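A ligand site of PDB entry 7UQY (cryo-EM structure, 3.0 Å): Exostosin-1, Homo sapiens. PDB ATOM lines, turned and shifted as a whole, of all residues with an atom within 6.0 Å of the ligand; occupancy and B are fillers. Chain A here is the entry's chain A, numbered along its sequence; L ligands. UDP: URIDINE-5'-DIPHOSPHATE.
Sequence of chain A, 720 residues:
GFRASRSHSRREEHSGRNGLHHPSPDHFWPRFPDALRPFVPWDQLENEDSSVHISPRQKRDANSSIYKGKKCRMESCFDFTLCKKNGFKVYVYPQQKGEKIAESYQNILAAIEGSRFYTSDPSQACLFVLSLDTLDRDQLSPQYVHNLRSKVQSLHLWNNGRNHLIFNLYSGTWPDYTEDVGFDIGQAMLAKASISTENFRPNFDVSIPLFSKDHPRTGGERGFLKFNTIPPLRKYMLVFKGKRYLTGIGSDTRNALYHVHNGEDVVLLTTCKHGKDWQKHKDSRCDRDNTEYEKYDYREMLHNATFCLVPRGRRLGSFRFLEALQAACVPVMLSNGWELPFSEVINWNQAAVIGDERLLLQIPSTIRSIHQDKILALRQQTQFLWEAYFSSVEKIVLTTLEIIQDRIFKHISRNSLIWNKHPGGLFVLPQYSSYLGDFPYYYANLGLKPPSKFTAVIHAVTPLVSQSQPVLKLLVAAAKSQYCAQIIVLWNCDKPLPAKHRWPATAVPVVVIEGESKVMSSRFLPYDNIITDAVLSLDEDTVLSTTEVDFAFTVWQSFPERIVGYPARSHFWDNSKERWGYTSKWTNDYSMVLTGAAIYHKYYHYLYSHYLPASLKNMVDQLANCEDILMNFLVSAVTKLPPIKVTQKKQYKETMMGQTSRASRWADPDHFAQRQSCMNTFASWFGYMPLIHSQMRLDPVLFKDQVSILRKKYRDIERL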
ATOM      1  N   SER A 212      35.412  33.692  -9.830  1.00  0.00           N
ATOM      2  CA  SER A 212      36.166  33.165  -8.707  1.00  0.00           C
ATOM      3  C   SER A 212      37.655  33.459  -8.862  1.00  0.00           C
ATOM      4  O   SER A 212      38.131  33.902  -9.912  1.00  0.00           O
ATOM      5  CB  SER A 212      35.954  31.652  -8.573  1.00  0.00           C
ATOM      6  OG  SER A 212      34.585  31.310  -8.700  1.00  0.00           O
ATOM      7  N   PHE A 240      18.293  23.212 -10.608  1.00  0.00           N
ATOM      8  CA  PHE A 240      18.944  24.098  -9.646  1.00  0.00           C
ATOM      9  C   PHE A 240      19.498  23.251  -8.508  1.00  0.00           C
ATOM     10  O   PHE A 240      18.833  22.316  -8.050  1.00  0.00           O
ATOM     11  CB  PHE A 240      17.966  25.148  -9.091  1.00  0.00           C
ATOM     12  CG  PHE A 240      18.558  25.990  -7.996  1.00  0.00           C
ATOM     13  CD1 PHE A 240      19.494  26.956  -8.287  1.00  0.00           C
ATOM     14  CD2 PHE A 240      18.187  25.795  -6.674  1.00  0.00           C
ATOM     15  CE1 PHE A 240      20.042  27.739  -7.284  1.00  0.00           C
ATOM     16  CE2 PHE A 240      18.733  26.555  -5.672  1.00  0.00           C
ATOM     17  CZ  PHE A 240      19.655  27.537  -5.975  1.00  0.00           C
ATOM     18  N   LYS A 241      20.696  23.594  -8.051  1.00  0.00           N
ATOM     19  CA  LYS A 241      21.302  22.911  -6.901  1.00  0.00           C
ATOM     20  C   LYS A 241      22.139  23.937  -6.140  1.00  0.00           C
ATOM     21  O   LYS A 241      23.314  24.161  -6.457  1.00  0.00           O
ATOM     22  CB  LYS A 241      22.129  21.704  -7.332  1.00  0.00           C
ATOM     23  CG  LYS A 241      22.747  20.916  -6.191  1.00  0.00           C
ATOM     24  CD  LYS A 241      23.435  19.639  -6.660  1.00  0.00           C
ATOM     25  CE  LYS A 241      23.833  18.764  -5.486  1.00  0.00           C
ATOM     26  NZ  LYS A 241      25.128  19.209  -4.898  1.00  0.00           N
ATOM     27  N   GLY A 242      21.528  24.553  -5.134  1.00  0.00           N
ATOM     28  CA  GLY A 242      22.197  25.626  -4.406  1.00  0.00           C
ATOM     29  C   GLY A 242      21.642  25.780  -3.012  1.00  0.00           C
ATOM     30  O   GLY A 242      20.618  25.196  -2.654  1.00  0.00           O
ATOM     31  N   LYS A 243      22.344  26.585  -2.225  1.00  0.00           N
ATOM     32  CA  LYS A 243      21.970  26.791  -0.841  1.00  0.00           C
ATOM     33  C   LYS A 243      20.742  27.689  -0.740  1.00  0.00           C
ATOM     34  O   LYS A 243      20.561  28.627  -1.510  1.00  0.00           O
ATOM     35  CB  LYS A 243      23.132  27.395  -0.046  1.00  0.00           C
ATOM     36  CG  LYS A 243      24.367  26.516   0.030  1.00  0.00           C
ATOM     37  CD  LYS A 243      25.452  27.194   0.843  1.00  0.00           C
ATOM     38  CE  LYS A 243      26.684  26.313   0.992  1.00  0.00           C
ATOM     39  NZ  LYS A 243      27.424  26.167  -0.294  1.00  0.00           N
ATOM     40  N   ARG A 244      19.892  27.382   0.243  1.00  0.00           N
ATOM     41  CA  ARG A 244      18.795  28.253   0.641  1.00  0.00           C
ATOM     42  C   ARG A 244      19.086  28.794   2.029  1.00  0.00           C
ATOM     43  O   ARG A 244      19.698  28.111   2.868  1.00  0.00           O
ATOM     44  CB  ARG A 244      17.446  27.517   0.628  1.00  0.00           C
ATOM     45  CG  ARG A 244      17.358  26.344   1.579  1.00  0.00           C
ATOM     46  CD  ARG A 244      15.925  25.918   1.811  1.00  0.00           C
ATOM     47  NE  ARG A 244      15.146  26.961   2.462  1.00  0.00           N
ATOM     48  CZ  ARG A 244      14.013  26.753   3.111  1.00  0.00           C
ATOM     49  NH1 ARG A 244      13.500  25.541   3.240  1.00  0.00           N
ATOM     50  NH2 ARG A 244      13.381  27.786   3.664  1.00  0.00           N
ATOM     51  N   TYR A 245      18.654  30.025   2.280  1.00  0.00           N
ATOM     52  CA  TYR A 245      19.046  30.763   3.474  1.00  0.00           C
ATOM     53  C   TYR A 245      17.839  30.913   4.386  1.00  0.00           C
ATOM     54  O   TYR A 245      16.791  31.402   3.968  1.00  0.00           O
ATOM     55  CB  TYR A 245      19.603  32.127   3.070  1.00  0.00           C
ATOM     56  CG  TYR A 245      20.923  32.035   2.337  1.00  0.00           C
ATOM     57  CD1 TYR A 245      21.662  30.860   2.349  1.00  0.00           C
ATOM     58  CD2 TYR A 245      21.409  33.108   1.597  1.00  0.00           C
ATOM     59  CE1 TYR A 245      22.863  30.765   1.674  1.00  0.00           C
ATOM     60  CE2 TYR A 245      22.602  33.014   0.918  1.00  0.00           C
ATOM     61  CZ  TYR A 245      23.331  31.850   0.954  1.00  0.00           C
ATOM     62  OH  TYR A 245      24.523  31.756   0.275  1.00  0.00           O
ATOM     63  N   ARG A 254      14.457  31.758  -3.365  1.00  0.00           N
ATOM     64  CA  ARG A 254      15.039  30.440  -3.213  1.00  0.00           C
ATOM     65  C   ARG A 254      14.158  29.534  -2.372  1.00  0.00           C
ATOM     66  O   ARG A 254      14.105  28.317  -2.614  1.00  0.00           O
ATOM     67  CB  ARG A 254      16.409  30.571  -2.552  1.00  0.00           C
ATOM     68  CG  ARG A 254      17.441  31.289  -3.415  1.00  0.00           C
ATOM     69  CD  ARG A 254      18.773  31.346  -2.700  1.00  0.00           C
ATOM     70  NE  ARG A 254      19.758  32.119  -3.448  1.00  0.00           N
ATOM     71  CZ  ARG A 254      20.567  31.609  -4.365  1.00  0.00           C
ATOM     72  NH1 ARG A 254      20.525  30.333  -4.693  1.00  0.00           N
ATOM     73  NH2 ARG A 254      21.459  32.405  -4.941  1.00  0.00           N
ATOM     74  N   HIS A 274      24.491  26.179   6.193  1.00  0.00           N
ATOM     75  CA  HIS A 274      25.374  27.309   5.968  1.00  0.00           C
ATOM     76  C   HIS A 274      25.976  27.799   7.280  1.00  0.00           C
ATOM     77  O   HIS A 274      26.023  29.012   7.553  1.00  0.00           O
ATOM     78  CB  HIS A 274      24.632  28.451   5.261  1.00  0.00           C
ATOM     79  CG  HIS A 274      25.540  29.463   4.628  1.00  0.00           C
ATOM     80  ND1 HIS A 274      26.247  29.202   3.465  1.00  0.00           N
ATOM     81  CD2 HIS A 274      25.865  30.721   4.992  1.00  0.00           C
ATOM     82  CE1 HIS A 274      26.954  30.273   3.149  1.00  0.00           C
ATOM     83  NE2 HIS A 274      26.743  31.209   4.053  1.00  0.00           N
ATOM     84  N   TYR A 293      19.154  16.333  -1.599  1.00  0.00           N
ATOM     85  CA  TYR A 293      20.312  17.028  -2.151  1.00  0.00           C
ATOM     86  C   TYR A 293      21.477  16.097  -2.478  1.00  0.00           C
ATOM     87  O   TYR A 293      22.331  16.469  -3.289  1.00  0.00           O
ATOM     88  CB  TYR A 293      20.771  18.094  -1.156  1.00  0.00           C
ATOM     89  CG  TYR A 293      21.517  19.264  -1.776  1.00  0.00           C
ATOM     90  CD1 TYR A 293      20.828  20.293  -2.397  1.00  0.00           C
ATOM     91  CD2 TYR A 293      22.895  19.344  -1.701  1.00  0.00           C
ATOM     92  CE1 TYR A 293      21.502  21.359  -2.948  1.00  0.00           C
ATOM     93  CE2 TYR A 293      23.578  20.409  -2.247  1.00  0.00           C
ATOM     94  CZ  TYR A 293      22.877  21.417  -2.872  1.00  0.00           C
ATOM     95  OH  TYR A 293      23.551  22.483  -3.423  1.00  0.00           O
ATOM     96  N   TYR A 298      26.451  18.175  -9.359  1.00  0.00           N
ATOM     97  CA  TYR A 298      26.238  19.519  -9.893  1.00  0.00           C
ATOM     98  C   TYR A 298      26.829  19.726 -11.273  1.00  0.00           C
ATOM     99  O   TYR A 298      26.301  20.535 -12.039  1.00  0.00           O
ATOM    100  CB  TYR A 298      26.816  20.569  -8.939  1.00  0.00           C
ATOM    101  CG  TYR A 298      26.360  21.981  -9.274  1.00  0.00           C
ATOM    102  CD1 TYR A 298      25.074  22.405  -8.969  1.00  0.00           C
ATOM    103  CD2 TYR A 298      27.212  22.874  -9.899  1.00  0.00           C
ATOM    104  CE1 TYR A 298      24.651  23.685  -9.277  1.00  0.00           C
ATOM    105  CE2 TYR A 298      26.803  24.156 -10.210  1.00  0.00           C
ATOM    106  CZ  TYR A 298      25.518  24.553  -9.893  1.00  0.00           C
ATOM    107  OH  TYR A 298      25.109  25.836 -10.205  1.00  0.00           O
ATOM    108  N   PRO A 311      19.259  32.495  -9.590  1.00  0.00           N
ATOM    109  CA  PRO A 311      18.501  33.377  -8.708  1.00  0.00           C
ATOM    110  C   PRO A 311      19.403  34.234  -7.832  1.00  0.00           C
ATOM    111  O   PRO A 311      20.610  34.012  -7.729  1.00  0.00           O
ATOM    112  CB  PRO A 311      17.664  32.406  -7.863  1.00  0.00           C
ATOM    113  CG  PRO A 311      18.495  31.172  -7.804  1.00  0.00           C
ATOM    114  CD  PRO A 311      19.309  31.115  -9.079  1.00  0.00           C
ATOM    115  N   ARG A 312      18.794  35.222  -7.202  1.00  0.00           N
ATOM    116  CA  ARG A 312      19.495  36.124  -6.291  1.00  0.00           C
ATOM    117  C   ARG A 312      19.714  35.443  -4.945  1.00  0.00           C
ATOM    118  O   ARG A 312      18.802  34.830  -4.388  1.00  0.00           O
ATOM    119  CB  ARG A 312      18.702  37.416  -6.111  1.00  0.00           C
ATOM    120  CG  ARG A 312      18.923  38.113  -4.785  1.00  0.00           C
ATOM    121  CD  ARG A 312      18.064  39.352  -4.669  1.00  0.00           C
ATOM    122  NE  ARG A 312      18.532  40.244  -3.606  1.00  0.00           N
ATOM    123  CZ  ARG A 312      17.959  41.395  -3.299  1.00  0.00           C
ATOM    124  NH1 ARG A 312      16.894  41.845  -3.947  1.00  0.00           N
ATOM    125  NH2 ARG A 312      18.471  42.124  -2.306  1.00  0.00           N
ATOM    126  N   GLY A 313      20.937  35.551  -4.428  1.00  0.00           N
ATOM    127  CA  GLY A 313      21.236  35.107  -3.081  1.00  0.00           C
ATOM    128  C   GLY A 313      21.440  36.282  -2.149  1.00  0.00           C
ATOM    129  O   GLY A 313      20.568  37.154  -2.050  1.00  0.00           O
ATOM    130  N   ARG A 314      22.578  36.314  -1.456  1.00  0.00           N
ATOM    131  CA  ARG A 314      22.943  37.510  -0.712  1.00  0.00           C
ATOM    132  C   ARG A 314      23.129  38.697  -1.651  1.00  0.00           C
ATOM    133  O   ARG A 314      22.670  39.818  -1.357  1.00  0.00           O
ATOM    134  CB  ARG A 314      24.219  37.267   0.096  1.00  0.00           C
ATOM    135  CG  ARG A 314      24.042  36.333   1.280  1.00  0.00           C
ATOM    136  CD  ARG A 314      22.832  36.711   2.106  1.00  0.00           C
ATOM    137  NE  ARG A 314      22.434  35.646   3.012  1.00  0.00           N
ATOM    138  CZ  ARG A 314      21.527  35.776   3.970  1.00  0.00           C
ATOM    139  NH1 ARG A 314      20.899  36.913   4.178  1.00  0.00           N
ATOM    140  NH2 ARG A 314      21.239  34.724   4.745  1.00  0.00           N
ATOM    141  N   ARG A 315      23.782  38.483  -2.782  1.00  0.00           N
ATOM    142  CA  ARG A 315      24.023  39.518  -3.766  1.00  0.00           C
ATOM    143  C   ARG A 315      23.292  39.169  -5.067  1.00  0.00           C
ATOM    144  O   ARG A 315      22.907  38.021  -5.298  1.00  0.00           O
ATOM    145  CB  ARG A 315      25.523  39.686  -4.029  1.00  0.00           C
ATOM    146  CG  ARG A 315      26.269  40.298  -2.863  1.00  0.00           C
ATOM    147  CD  ARG A 315      27.754  40.432  -3.151  1.00  0.00           C
ATOM    148  NE  ARG A 315      28.437  41.177  -2.092  1.00  0.00           N
ATOM    149  CZ  ARG A 315      28.805  40.658  -0.931  1.00  0.00           C
ATOM    150  NH1 ARG A 315      28.573  39.390  -0.635  1.00  0.00           N
ATOM    151  NH2 ARG A 315      29.416  41.429  -0.037  1.00  0.00           N
ATOM    152  N   GLY A 317      24.368  39.160  -8.225  1.00  0.00           N
ATOM    153  CA  GLY A 317      25.114  38.247  -9.067  1.00  0.00           C
ATOM    154  C   GLY A 317      25.510  36.969  -8.360  1.00  0.00           C
ATOM    155  O   GLY A 317      25.369  36.828  -7.145  1.00  0.00           O
ATOM    156  N   SER A 318      26.009  36.021  -9.145  1.00  0.00           N
ATOM    157  CA  SER A 318      26.448  34.740  -8.616  1.00  0.00           C
ATOM    158  C   SER A 318      27.396  34.099  -9.608  1.00  0.00           C
ATOM    159  O   SER A 318      27.421  34.450 -10.796  1.00  0.00           O
ATOM    160  CB  SER A 318      25.249  33.820  -8.325  1.00  0.00           C
ATOM    161  OG  SER A 318      24.805  33.171  -9.503  1.00  0.00           O
ATOM    162  N   PHE A 319      28.183  33.149  -9.118  1.00  0.00           N
ATOM    163  CA  PHE A 319      29.094  32.389  -9.953  1.00  0.00           C
ATOM    164  C   PHE A 319      28.374  31.440 -10.886  1.00  0.00           C
ATOM    165  O   PHE A 319      28.984  30.977 -11.865  1.00  0.00           O
ATOM    166  CB  PHE A 319      30.066  31.587  -9.084  1.00  0.00           C
ATOM    167  CG  PHE A 319      30.877  32.428  -8.142  1.00  0.00           C
ATOM    168  CD1 PHE A 319      32.089  32.964  -8.531  1.00  0.00           C
ATOM    169  CD2 PHE A 319      30.423  32.683  -6.854  1.00  0.00           C
ATOM    170  CE1 PHE A 319      32.836  33.734  -7.662  1.00  0.00           C
ATOM    171  CE2 PHE A 319      31.165  33.440  -5.980  1.00  0.00           C
ATOM    172  CZ  PHE A 319      32.373  33.972  -6.386  1.00  0.00           C
ATOM    173  N   ARG A 320      27.107  31.130 -10.614  1.00  0.00           N
ATOM    174  CA  ARG A 320      26.399  30.127 -11.403  1.00  0.00           C
ATOM    175  C   ARG A 320      26.149  30.615 -12.814  1.00  0.00           C
ATOM    176  O   ARG A 320      25.962  29.821 -13.732  1.00  0.00           O
ATOM    177  CB  ARG A 320      25.077  29.783 -10.729  1.00  0.00           C
ATOM    178  CG  ARG A 320      24.259  28.709 -11.429  1.00  0.00           C
ATOM    179  CD  ARG A 320      23.100  28.288 -10.538  1.00  0.00           C
ATOM    180  NE  ARG A 320      23.614  27.636  -9.350  1.00  0.00           N
ATOM    181  CZ  ARG A 320      23.625  28.156  -8.130  1.00  0.00           C
ATOM    182  NH1 ARG A 320      23.188  29.383  -7.895  1.00  0.00           N
ATOM    183  NH2 ARG A 320      24.077  27.425  -7.116  1.00  0.00           N
ATOM    184  N   GLU A 323      29.082  29.728 -14.982  1.00  0.00           N
ATOM    185  CA  GLU A 323      29.103  28.282 -15.146  1.00  0.00           C
ATOM    186  C   GLU A 323      27.973  27.801 -16.061  1.00  0.00           C
ATOM    187  O   GLU A 323      28.133  26.801 -16.763  1.00  0.00           O
ATOM    188  CB  GLU A 323      29.009  27.590 -13.781  1.00  0.00           C
ATOM    189  CG  GLU A 323      30.272  27.701 -12.953  1.00  0.00           C
ATOM    190  CD  GLU A 323      30.283  26.759 -11.767  1.00  0.00           C
ATOM    191  OE1 GLU A 323      29.403  25.879 -11.703  1.00  0.00           O
ATOM    192  OE2 GLU A 323      31.175  26.903 -10.905  1.00  0.00           O
HETATM  193  N1  UDP L   1      28.521  24.458  -6.249  1.00  0.00           N
HETATM  194  C2  UDP L   1      28.980  23.211  -6.606  1.00  0.00           C
HETATM  195  N3  UDP L   1      28.236  22.156  -6.115  1.00  0.00           N
HETATM  196  C4  UDP L   1      27.112  22.247  -5.323  1.00  0.00           C
HETATM  197  C5  UDP L   1      26.711  23.577  -4.992  1.00  0.00           C
HETATM  198  C6  UDP L   1      27.411  24.620  -5.464  1.00  0.00           C
HETATM  199  O2  UDP L   1      29.968  23.034  -7.305  1.00  0.00           O
HETATM  200  O4  UDP L   1      26.550  21.205  -4.948  1.00  0.00           O
HETATM  201  C1' UDP L   1      29.272  25.625  -6.743  1.00  0.00           C
HETATM  202  C2' UDP L   1      28.715  26.177  -8.056  1.00  0.00           C
HETATM  203  O2' UDP L   1      29.377  25.578  -9.163  1.00  0.00           O
HETATM  204  C3' UDP L   1      29.072  27.665  -7.921  1.00  0.00           C
HETATM  205  C4' UDP L   1      28.881  27.916  -6.437  1.00  0.00           C
HETATM  206  O4' UDP L   1      29.174  26.666  -5.786  1.00  0.00           O
HETATM  207  O3' UDP L   1      30.413  27.925  -8.314  1.00  0.00           O
HETATM  208  C5' UDP L   1      27.494  28.384  -6.028  1.00  0.00           C
HETATM  209  O5' UDP L   1      27.503  28.626  -4.611  1.00  0.00           O
HETATM  210  PA  UDP L   1      26.158  28.888  -3.820  1.00  0.00           P
HETATM  211  O1A UDP L   1      25.021  28.032  -4.376  1.00  0.00           O
HETATM  212  O2A UDP L   1      26.466  28.744  -2.379  1.00  0.00           O
HETATM  213  O3A UDP L   1      25.785  30.396  -4.160  1.00  0.00           O
HETATM  214  PB  UDP L   1      24.696  31.223  -3.354  1.00  0.00           P
HETATM  215  O1B UDP L   1      23.729  30.154  -2.870  1.00  0.00           O
HETATM  216  O2B UDP L   1      25.495  31.777  -2.175  1.00  0.00           O
HETATM  217  O3B UDP L   1      24.062  32.270  -4.198  1.00  0.00           O
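Gly 242 touches the ligand (CA to O1A, 3.7 Å). OH of Tyr 293 touches O4 of the ligand (3.6 Å). Tyr 298 touches the ligand (CE2 to O2', 3.1 Å). Phe 319 touches the ligand. Hydrophobic or aromatic side chains that line the ligand: Tyr 245, Tyr 298 and Phe 319. Of the 21 residues printed, 10 come within 4 Å of the ligand.
The backbone carbonyl oxygen (O) of Lys 241 sits at hydrogen-bond distance from the guanidinium group (NH2) of Arg 320. NH2 of Arg 254 sits at hydrogen-bond distance from O of Pro 311 (3.3 Å). The guanidinium group of Arg 320 sits at hydrogen-bond distance from the side-chain hydroxyl of Tyr 298 (2.5 Å). OG of Ser 318 sits close to N of Arg 320, at 3.3 Å. The side-chain hydroxyl (OH) of Tyr 293 lies within hydrogen-bond range of the backbone NH (N) of Gly 242. The guanidinium group of Arg 254 sits at hydrogen-bond distance from the backbone carbonyl oxygen of Arg 312, 3.0 Å away. The backbone carbonyl oxygen of Lys 241 lies close to the side-chain hydroxyl of Tyr 293, 3.5 Å away.
The side-chain amino group (NZ) of Lys 243 is in salt-bridge range of an oxygen (O2A) of the ligand. An oxygen (O2B) of the ligand lies within hydrogen-bond range of the side-chain hydroxyl (OH) of Tyr 245 (2.6 Å). An oxygen (O4) of the ligand sits at hydrogen-bond distance from the side-chain amino group of Lys 241 (2.5 Å). OE1 of Glu 323 lies within hydrogen-bond range of O2' of the ligand, 2.6 Å away. NH2 of Arg 320 is in salt-bridge range of O1A of the ligand, at 3.0 Å. O3B of the ligand lies within salt-bridge range of NH2 of Arg 254 (2.7 Å).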
